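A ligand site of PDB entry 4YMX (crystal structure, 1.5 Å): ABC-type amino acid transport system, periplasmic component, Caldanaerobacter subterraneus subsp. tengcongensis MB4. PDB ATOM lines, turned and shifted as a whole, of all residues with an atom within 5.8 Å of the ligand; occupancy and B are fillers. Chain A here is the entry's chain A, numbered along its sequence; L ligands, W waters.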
ATOM      1  N   THR A  43      29.228 -29.967 -10.626  1.00  0.00           N
ATOM      2  CA  THR A  43      28.706 -28.866  -9.832  1.00  0.00           C
ATOM      3  C   THR A  43      29.771 -28.347  -8.886  1.00  0.00           C
ATOM      4  O   THR A  43      30.845 -28.942  -8.761  1.00  0.00           O
ATOM      5  CB  THR A  43      27.422 -29.250  -9.052  1.00  0.00           C
ATOM      6  OG1 THR A  43      26.806 -28.055  -8.570  1.00  0.00           O
ATOM      7  CG2 THR A  43      27.717 -30.183  -7.864  1.00  0.00           C
ATOM      8  N   SER A  44      29.488 -27.217  -8.241  1.00  0.00           N
ATOM      9  CA  SER A  44      30.338 -26.685  -7.193  1.00  0.00           C
ATOM     10  C   SER A  44      29.477 -26.653  -5.935  1.00  0.00           C
ATOM     11  O   SER A  44      28.612 -25.781  -5.799  1.00  0.00           O
ATOM     12  CB  SER A  44      30.820 -25.276  -7.551  1.00  0.00           C
ATOM     13  OG  SER A  44      31.655 -24.738  -6.527  1.00  0.00           O
ATOM     14  N   ALA A  45      29.682 -27.614  -5.044  1.00  0.00           N
ATOM     15  CA  ALA A  45      28.759 -27.824  -3.922  1.00  0.00           C
ATOM     16  C   ALA A  45      29.119 -26.992  -2.693  1.00  0.00           C
ATOM     17  O   ALA A  45      29.298 -27.505  -1.572  1.00  0.00           O
ATOM     18  CB  ALA A  45      28.663 -29.314  -3.573  1.00  0.00           C
ATOM     19  N   ASP A  46      29.192 -25.681  -2.919  1.00  0.00           N
ATOM     20  CA  ASP A  46      29.457 -24.684  -1.910  1.00  0.00           C
ATOM     21  C   ASP A  46      28.343 -23.644  -1.904  1.00  0.00           C
ATOM     22  O   ASP A  46      28.543 -22.512  -1.492  1.00  0.00           O
ATOM     23  CB  ASP A  46      30.782 -23.982  -2.249  1.00  0.00           C
ATOM     24  CG  ASP A  46      30.773 -23.323  -3.637  1.00  0.00           C
ATOM     25  OD1 ASP A  46      29.851 -23.573  -4.455  1.00  0.00           O
ATOM     26  OD2 ASP A  46      31.700 -22.549  -3.919  1.00  0.00           O
ATOM     27  N   PHE A  47      27.167 -24.050  -2.375  1.00  0.00           N
ATOM     28  CA  PHE A  47      26.145 -23.101  -2.798  1.00  0.00           C
ATOM     29  C   PHE A  47      24.763 -23.524  -2.317  1.00  0.00           C
ATOM     30  O   PHE A  47      23.848 -23.730  -3.124  1.00  0.00           O
ATOM     31  CB  PHE A  47      26.175 -23.034  -4.335  1.00  0.00           C
ATOM     32  CG  PHE A  47      25.832 -21.685  -4.935  1.00  0.00           C
ATOM     33  CD1 PHE A  47      24.756 -21.551  -5.809  1.00  0.00           C
ATOM     34  CD2 PHE A  47      26.594 -20.555  -4.649  1.00  0.00           C
ATOM     35  CE1 PHE A  47      24.459 -20.337  -6.412  1.00  0.00           C
ATOM     36  CE2 PHE A  47      26.302 -19.338  -5.240  1.00  0.00           C
ATOM     37  CZ  PHE A  47      25.229 -19.214  -6.113  1.00  0.00           C
ATOM     38  N   GLU A  51      23.258 -26.579  -4.163  1.00  0.00           N
ATOM     39  CA  GLU A  51      24.093 -27.759  -4.008  1.00  0.00           C
ATOM     40  C   GLU A  51      25.034 -27.546  -2.850  1.00  0.00           C
ATOM     41  O   GLU A  51      25.699 -26.505  -2.747  1.00  0.00           O
ATOM     42  CB  GLU A  51      24.887 -28.064  -5.277  1.00  0.00           C
ATOM     43  CG  GLU A  51      25.618 -26.866  -5.837  1.00  0.00           C
ATOM     44  CD  GLU A  51      24.819 -26.164  -6.896  1.00  0.00           C
ATOM     45  OE1 GLU A  51      23.964 -26.842  -7.504  1.00  0.00           O
ATOM     46  OE2 GLU A  51      25.048 -24.963  -7.125  1.00  0.00           O
ATOM     47  N   PHE A  88      33.879 -23.886  -9.004  1.00  0.00           N
ATOM     48  CA  PHE A  88      32.934 -23.365  -9.997  1.00  0.00           C
ATOM     49  C   PHE A  88      33.611 -22.970 -11.311  1.00  0.00           C
ATOM     50  O   PHE A  88      33.112 -23.265 -12.409  1.00  0.00           O
ATOM     51  CB  PHE A  88      32.149 -22.179  -9.440  1.00  0.00           C
ATOM     52  CG  PHE A  88      31.143 -21.608 -10.410  1.00  0.00           C
ATOM     53  CD1 PHE A  88      29.854 -22.136 -10.494  1.00  0.00           C
ATOM     54  CD2 PHE A  88      31.482 -20.564 -11.259  1.00  0.00           C
ATOM     55  CE1 PHE A  88      28.926 -21.613 -11.398  1.00  0.00           C
ATOM     56  CE2 PHE A  88      30.561 -20.039 -12.151  1.00  0.00           C
ATOM     57  CZ  PHE A  88      29.275 -20.564 -12.212  1.00  0.00           C
ATOM     58  N   LEU A  91      33.927 -25.570 -14.114  1.00  0.00           N
ATOM     59  CA  LEU A  91      32.740 -26.271 -14.632  1.00  0.00           C
ATOM     60  C   LEU A  91      32.588 -26.180 -16.150  1.00  0.00           C
ATOM     61  O   LEU A  91      32.414 -27.207 -16.818  1.00  0.00           O
ATOM     62  CB  LEU A  91      31.459 -25.788 -13.939  1.00  0.00           C
ATOM     63  CG  LEU A  91      31.369 -26.225 -12.472  1.00  0.00           C
ATOM     64  CD1 LEU A  91      30.288 -25.412 -11.792  1.00  0.00           C
ATOM     65  CD2 LEU A  91      31.073 -27.709 -12.359  1.00  0.00           C
ATOM     66  N   ALA A 105      24.589 -25.776 -11.408  1.00  0.00           N
ATOM     67  CA  ALA A 105      25.338 -25.130 -10.330  1.00  0.00           C
ATOM     68  C   ALA A 105      24.888 -23.696 -10.109  1.00  0.00           C
ATOM     69  O   ALA A 105      25.717 -22.782  -9.985  1.00  0.00           O
ATOM     70  CB  ALA A 105      26.839 -25.178 -10.637  1.00  0.00           C
ATOM     71  N   GLY A 106      23.576 -23.479 -10.085  1.00  0.00           N
ATOM     72  CA  GLY A 106      23.027 -22.141  -9.994  1.00  0.00           C
ATOM     73  C   GLY A 106      23.654 -21.217 -11.035  1.00  0.00           C
ATOM     74  O   GLY A 106      23.973 -20.052 -10.767  1.00  0.00           O
ATOM     75  N   MET A 107      23.857 -21.759 -12.243  1.00  0.00           N
ATOM     76  CA  MET A 107      24.669 -21.109 -13.242  1.00  0.00           C
ATOM     77  C   MET A 107      23.858 -20.235 -14.185  1.00  0.00           C
ATOM     78  O   MET A 107      22.894 -20.680 -14.801  1.00  0.00           O
ATOM     79  CB  MET A 107      25.464 -22.141 -14.042  1.00  0.00           C
ATOM     80  CG  MET A 107      26.313 -21.501 -15.124  1.00  0.00           C
ATOM     81  SD  MET A 107      27.334 -22.649 -16.051  1.00  0.00           S
ATOM     82  CE  MET A 107      28.616 -23.004 -14.849  1.00  0.00           C
ATOM     83  N   THR A 108      24.275 -18.982 -14.297  1.00  0.00           N
ATOM     84  CA  THR A 108      23.540 -18.006 -15.106  1.00  0.00           C
ATOM     85  C   THR A 108      23.877 -18.164 -16.587  1.00  0.00           C
ATOM     86  O   THR A 108      25.039 -18.232 -16.962  1.00  0.00           O
ATOM     87  CB  THR A 108      23.847 -16.589 -14.640  1.00  0.00           C
ATOM     88  OG1 THR A 108      23.472 -16.459 -13.263  1.00  0.00           O
ATOM     89  CG2 THR A 108      23.082 -15.560 -15.469  1.00  0.00           C
ATOM     90  N   ARG A 113      28.861 -16.847 -21.883  1.00  0.00           N
ATOM     91  CA  ARG A 113      28.950 -18.293 -21.731  1.00  0.00           C
ATOM     92  C   ARG A 113      28.292 -19.060 -22.872  1.00  0.00           C
ATOM     93  O   ARG A 113      28.735 -20.156 -23.210  1.00  0.00           O
ATOM     94  CB  ARG A 113      28.339 -18.713 -20.397  1.00  0.00           C
ATOM     95  CG  ARG A 113      29.184 -18.332 -19.199  1.00  0.00           C
ATOM     96  CD  ARG A 113      28.380 -18.452 -17.941  1.00  0.00           C
ATOM     97  NE  ARG A 113      29.179 -18.105 -16.777  1.00  0.00           N
ATOM     98  CZ  ARG A 113      28.676 -17.917 -15.564  1.00  0.00           C
ATOM     99  NH1 ARG A 113      27.375 -18.049 -15.350  1.00  0.00           N
ATOM    100  NH2 ARG A 113      29.486 -17.621 -14.542  1.00  0.00           N
ATOM    101  N   SER A 126      17.445 -15.327  -9.869  1.00  0.00           N
ATOM    102  CA  SER A 126      18.434 -15.023  -8.846  1.00  0.00           C
ATOM    103  C   SER A 126      18.708 -13.528  -8.777  1.00  0.00           C
ATOM    104  O   SER A 126      18.380 -12.771  -9.700  1.00  0.00           O
ATOM    105  CB  SER A 126      19.751 -15.794  -9.081  1.00  0.00           C
ATOM    106  OG  SER A 126      20.382 -15.388 -10.284  1.00  0.00           O
ATOM    107  N   GLN A 128      21.811 -10.704  -7.121  1.00  0.00           N
ATOM    108  CA  GLN A 128      23.068 -10.413  -6.424  1.00  0.00           C
ATOM    109  C   GLN A 128      22.811  -9.504  -5.234  1.00  0.00           C
ATOM    110  O   GLN A 128      22.035  -8.552  -5.324  1.00  0.00           O
ATOM    111  CB  GLN A 128      24.052  -9.709  -7.365  1.00  0.00           C
ATOM    112  CG  GLN A 128      24.419 -10.514  -8.578  1.00  0.00           C
ATOM    113  CD  GLN A 128      25.069 -11.828  -8.223  1.00  0.00           C
ATOM    114  OE1 GLN A 128      26.034 -11.863  -7.457  1.00  0.00           O
ATOM    115  NE2 GLN A 128      24.534 -12.923  -8.766  1.00  0.00           N
ATOM    116  N   GLN A 152      33.578 -15.090  -5.961  1.00  0.00           N
ATOM    117  CA  GLN A 152      33.935 -16.388  -6.496  1.00  0.00           C
ATOM    118  C   GLN A 152      34.450 -16.235  -7.934  1.00  0.00           C
ATOM    119  O   GLN A 152      33.811 -15.612  -8.777  1.00  0.00           O
ATOM    120  CB  GLN A 152      32.747 -17.354  -6.443  1.00  0.00           C
ATOM    121  CG  GLN A 152      33.047 -18.730  -7.012  1.00  0.00           C
ATOM    122  CD  GLN A 152      32.003 -19.747  -6.634  1.00  0.00           C
ATOM    123  OE1 GLN A 152      30.792 -19.488  -6.738  1.00  0.00           O
ATOM    124  NE2 GLN A 152      32.458 -20.896  -6.153  1.00  0.00           N
ATOM    125  N   GLY A 154      35.103 -16.595 -11.642  1.00  0.00           N
ATOM    126  CA  GLY A 154      34.399 -17.107 -12.805  1.00  0.00           C
ATOM    127  C   GLY A 154      32.903 -16.847 -12.774  1.00  0.00           C
ATOM    128  O   GLY A 154      32.157 -17.376 -13.594  1.00  0.00           O
ATOM    129  N   THR A 155      32.461 -16.013 -11.844  1.00  0.00           N
ATOM    130  CA  THR A 155      31.032 -15.794 -11.636  1.00  0.00           C
ATOM    131  C   THR A 155      30.513 -14.425 -12.048  1.00  0.00           C
ATOM    132  O   THR A 155      31.265 -13.463 -12.219  1.00  0.00           O
ATOM    133  CB  THR A 155      30.618 -16.004 -10.166  1.00  0.00           C
ATOM    134  OG1 THR A 155      31.257 -15.023  -9.328  1.00  0.00           O
ATOM    135  CG2 THR A 155      30.968 -17.414  -9.688  1.00  0.00           C
ATOM    136  N   THR A 156      29.183 -14.337 -12.151  1.00  0.00           N
ATOM    137  CA  THR A 156      28.546 -13.046 -12.345  1.00  0.00           C
ATOM    138  C   THR A 156      28.709 -12.153 -11.113  1.00  0.00           C
ATOM    139  O   THR A 156      28.703 -10.921 -11.224  1.00  0.00           O
ATOM    140  CB  THR A 156      27.054 -13.206 -12.635  1.00  0.00           C
ATOM    141  OG1 THR A 156      26.462 -13.978 -11.587  1.00  0.00           O
ATOM    142  CG2 THR A 156      26.866 -13.918 -13.973  1.00  0.00           C
ATOM    143  N   SER A 157      28.874 -12.757  -9.941  1.00  0.00           N
ATOM    144  CA  SER A 157      29.146 -11.986  -8.726  1.00  0.00           C
ATOM    145  C   SER A 157      30.477 -11.266  -8.876  1.00  0.00           C
ATOM    146  O   SER A 157      30.584 -10.071  -8.566  1.00  0.00           O
ATOM    147  CB  SER A 157      29.176 -12.914  -7.511  1.00  0.00           C
ATOM    148  OG  SER A 157      27.939 -13.628  -7.396  1.00  0.00           O
ATOM    149  N   VAL A 175      32.831 -20.489  -2.373  1.00  0.00           N
ATOM    150  CA  VAL A 175      32.061 -19.508  -1.617  1.00  0.00           C
ATOM    151  C   VAL A 175      32.308 -19.620  -0.112  1.00  0.00           C
ATOM    152  O   VAL A 175      32.303 -18.608   0.598  1.00  0.00           O
ATOM    153  CB  VAL A 175      30.561 -19.651  -1.930  1.00  0.00           C
ATOM    154  CG1 VAL A 175      29.730 -18.725  -1.065  1.00  0.00           C
ATOM    155  CG2 VAL A 175      30.316 -19.361  -3.409  1.00  0.00           C
ATOM    156  N   GLU A 193      24.806 -14.458  -4.416  1.00  0.00           N
ATOM    157  CA  GLU A 193      23.357 -14.495  -4.592  1.00  0.00           C
ATOM    158  C   GLU A 193      22.622 -14.491  -3.266  1.00  0.00           C
ATOM    159  O   GLU A 193      23.079 -15.078  -2.269  1.00  0.00           O
ATOM    160  CB  GLU A 193      22.947 -15.685  -5.451  1.00  0.00           C
ATOM    161  CG  GLU A 193      22.832 -15.334  -6.913  1.00  0.00           C
ATOM    162  CD  GLU A 193      23.490 -16.353  -7.805  1.00  0.00           C
ATOM    163  OE1 GLU A 193      24.689 -16.207  -8.082  1.00  0.00           O
ATOM    164  OE2 GLU A 193      22.787 -17.279  -8.246  1.00  0.00           O
ATOM    165  N   GLY A 221      19.395 -15.330 -13.038  1.00  0.00           N
ATOM    166  CA  GLY A 221      18.731 -16.600 -13.280  1.00  0.00           C
ATOM    167  C   GLY A 221      19.703 -17.760 -13.356  1.00  0.00           C
ATOM    168  O   GLY A 221      20.910 -17.575 -13.548  1.00  0.00           O
ATOM    169  N   SER A 222      19.169 -18.965 -13.217  1.00  0.00           N
ATOM    170  CA  SER A 222      19.962 -20.189 -13.323  1.00  0.00           C
ATOM    171  C   SER A 222      19.400 -21.142 -14.379  1.00  0.00           C
ATOM    172  O   SER A 222      18.185 -21.242 -14.568  1.00  0.00           O
ATOM    173  CB  SER A 222      20.017 -20.903 -11.972  1.00  0.00           C
ATOM    174  OG  SER A 222      20.596 -20.037 -11.013  1.00  0.00           O
HETATM  175  N1  LIG L   1      24.981 -17.459 -10.587  1.00  0.00           N
HETATM  176  C1  LIG L   1      26.421 -17.097 -10.549  1.00  0.00           C
HETATM  177  C2  LIG L   1      27.098 -17.442 -11.861  1.00  0.00           C
HETATM  178  O1  LIG L   1      26.499 -18.077 -12.729  1.00  0.00           O
HETATM  179  C3  LIG L   1      27.122 -17.821  -9.392  1.00  0.00           C
HETATM  180  C4  LIG L   1      26.943 -19.322  -9.411  1.00  0.00           C
HETATM  181  C5  LIG L   1      27.869 -20.013  -8.430  1.00  0.00           C
HETATM  182  N2  LIG L   1      27.474 -21.396  -8.213  1.00  0.00           N
HETATM  183  C6  LIG L   1      28.101 -22.240  -7.399  1.00  0.00           C
HETATM  184  N3  LIG L   1      29.167 -21.858  -6.710  1.00  0.00           N
HETATM  185  N4  LIG L   1      27.655 -23.478  -7.275  1.00  0.00           N
HETATM  186  O2  LIG L   1      28.260 -17.084 -12.082  1.00  0.00           O
HETATM  187  O   HOH W   1      21.953 -17.482 -10.750  1.00  0.00           O
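The backbone NH (N) of Thr 156 is in hydrogen-bond range of an oxygen (O2) of the ligand.
The side-chain carboxylate of Glu 51 lies within salt-bridge range of a nitrogen (N4) of the ligand.
The side-chain hydroxyl (OG1) of Thr 108 is in hydrogen-bond range of a nitrogen (N1) of the ligand (3.2 Å).
An oxygen (O1) of the ligand lies within salt-bridge range of the guanidinium group (NH1) of Arg 113.
N4 of the ligand lies within hydrogen-bond range of O of Ser 44, at 2.9 Å.
N of Thr 108 sits at hydrogen-bond distance from O1 of the ligand (2.9 Å).
The side-chain amide oxygen (OE1) of Gln 152 lies within hydrogen-bond range of a nitrogen (N3) of the ligand (2.9 Å).
O of Gly 106 is in hydrogen-bond range of N1 of the ligand (2.8 Å).
The side-chain carboxylate (OE1) of Glu 193 lies within salt-bridge range of a nitrogen (N1) of the ligand.
N3 of the ligand lies within salt-bridge range of OD1 of Asp 46, at 2.9 Å.
N2 of the ligand is in hydrogen-bond range of O of Ala 105 (2.9 Å).
O of Thr 108 is in hydrogen-bond range of NH1 of Arg 113 (2.8 Å).
The side-chain carboxylate (OD2) of Asp 46 sits at hydrogen-bond distance from the backbone NH (N) of Val 175 (2.8 Å).
OG of Ser 44 is in hydrogen-bond range of N of Phe 88, 3.4 Å away.
The side-chain hydroxyl (OG) of Ser 44 is in hydrogen-bond range of the side-chain carboxylate (OD1) of Asp 46 (3.0 Å).
The backbone carbonyl oxygen of Gln 152 is in hydrogen-bond range of the side-chain hydroxyl of Thr 155, at 2.7 Å.
The backbone carbonyl oxygen (O) of Gly 106 lies close to the side-chain hydroxyl (OG) of Ser 222 (3.4 Å).
The guanidinium group of Arg 113 lies within hydrogen-bond range of the backbone carbonyl oxygen of Gly 154 (2.8 Å).
The side-chain hydroxyl (OG1) of Thr 108 sits at hydrogen-bond distance from the backbone carbonyl oxygen (O) of Gly 221 (2.8 Å).
CB of Phe 47 touches N4 of the ligand (3.3 Å).
CD1 of Phe 88 touches N2 of the ligand, 3.4 Å away.
Met 107 touches the ligand (CA to O1, 3.6 Å).
CA of Thr 155 touches O2 of the ligand, at 3.1 Å.
Hydrophobic or aromatic side chains that line the ligand: Phe 47, Phe 88 and Ala 105.
Of the 24 residues printed, 14 come within 4 Å of the ligand.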
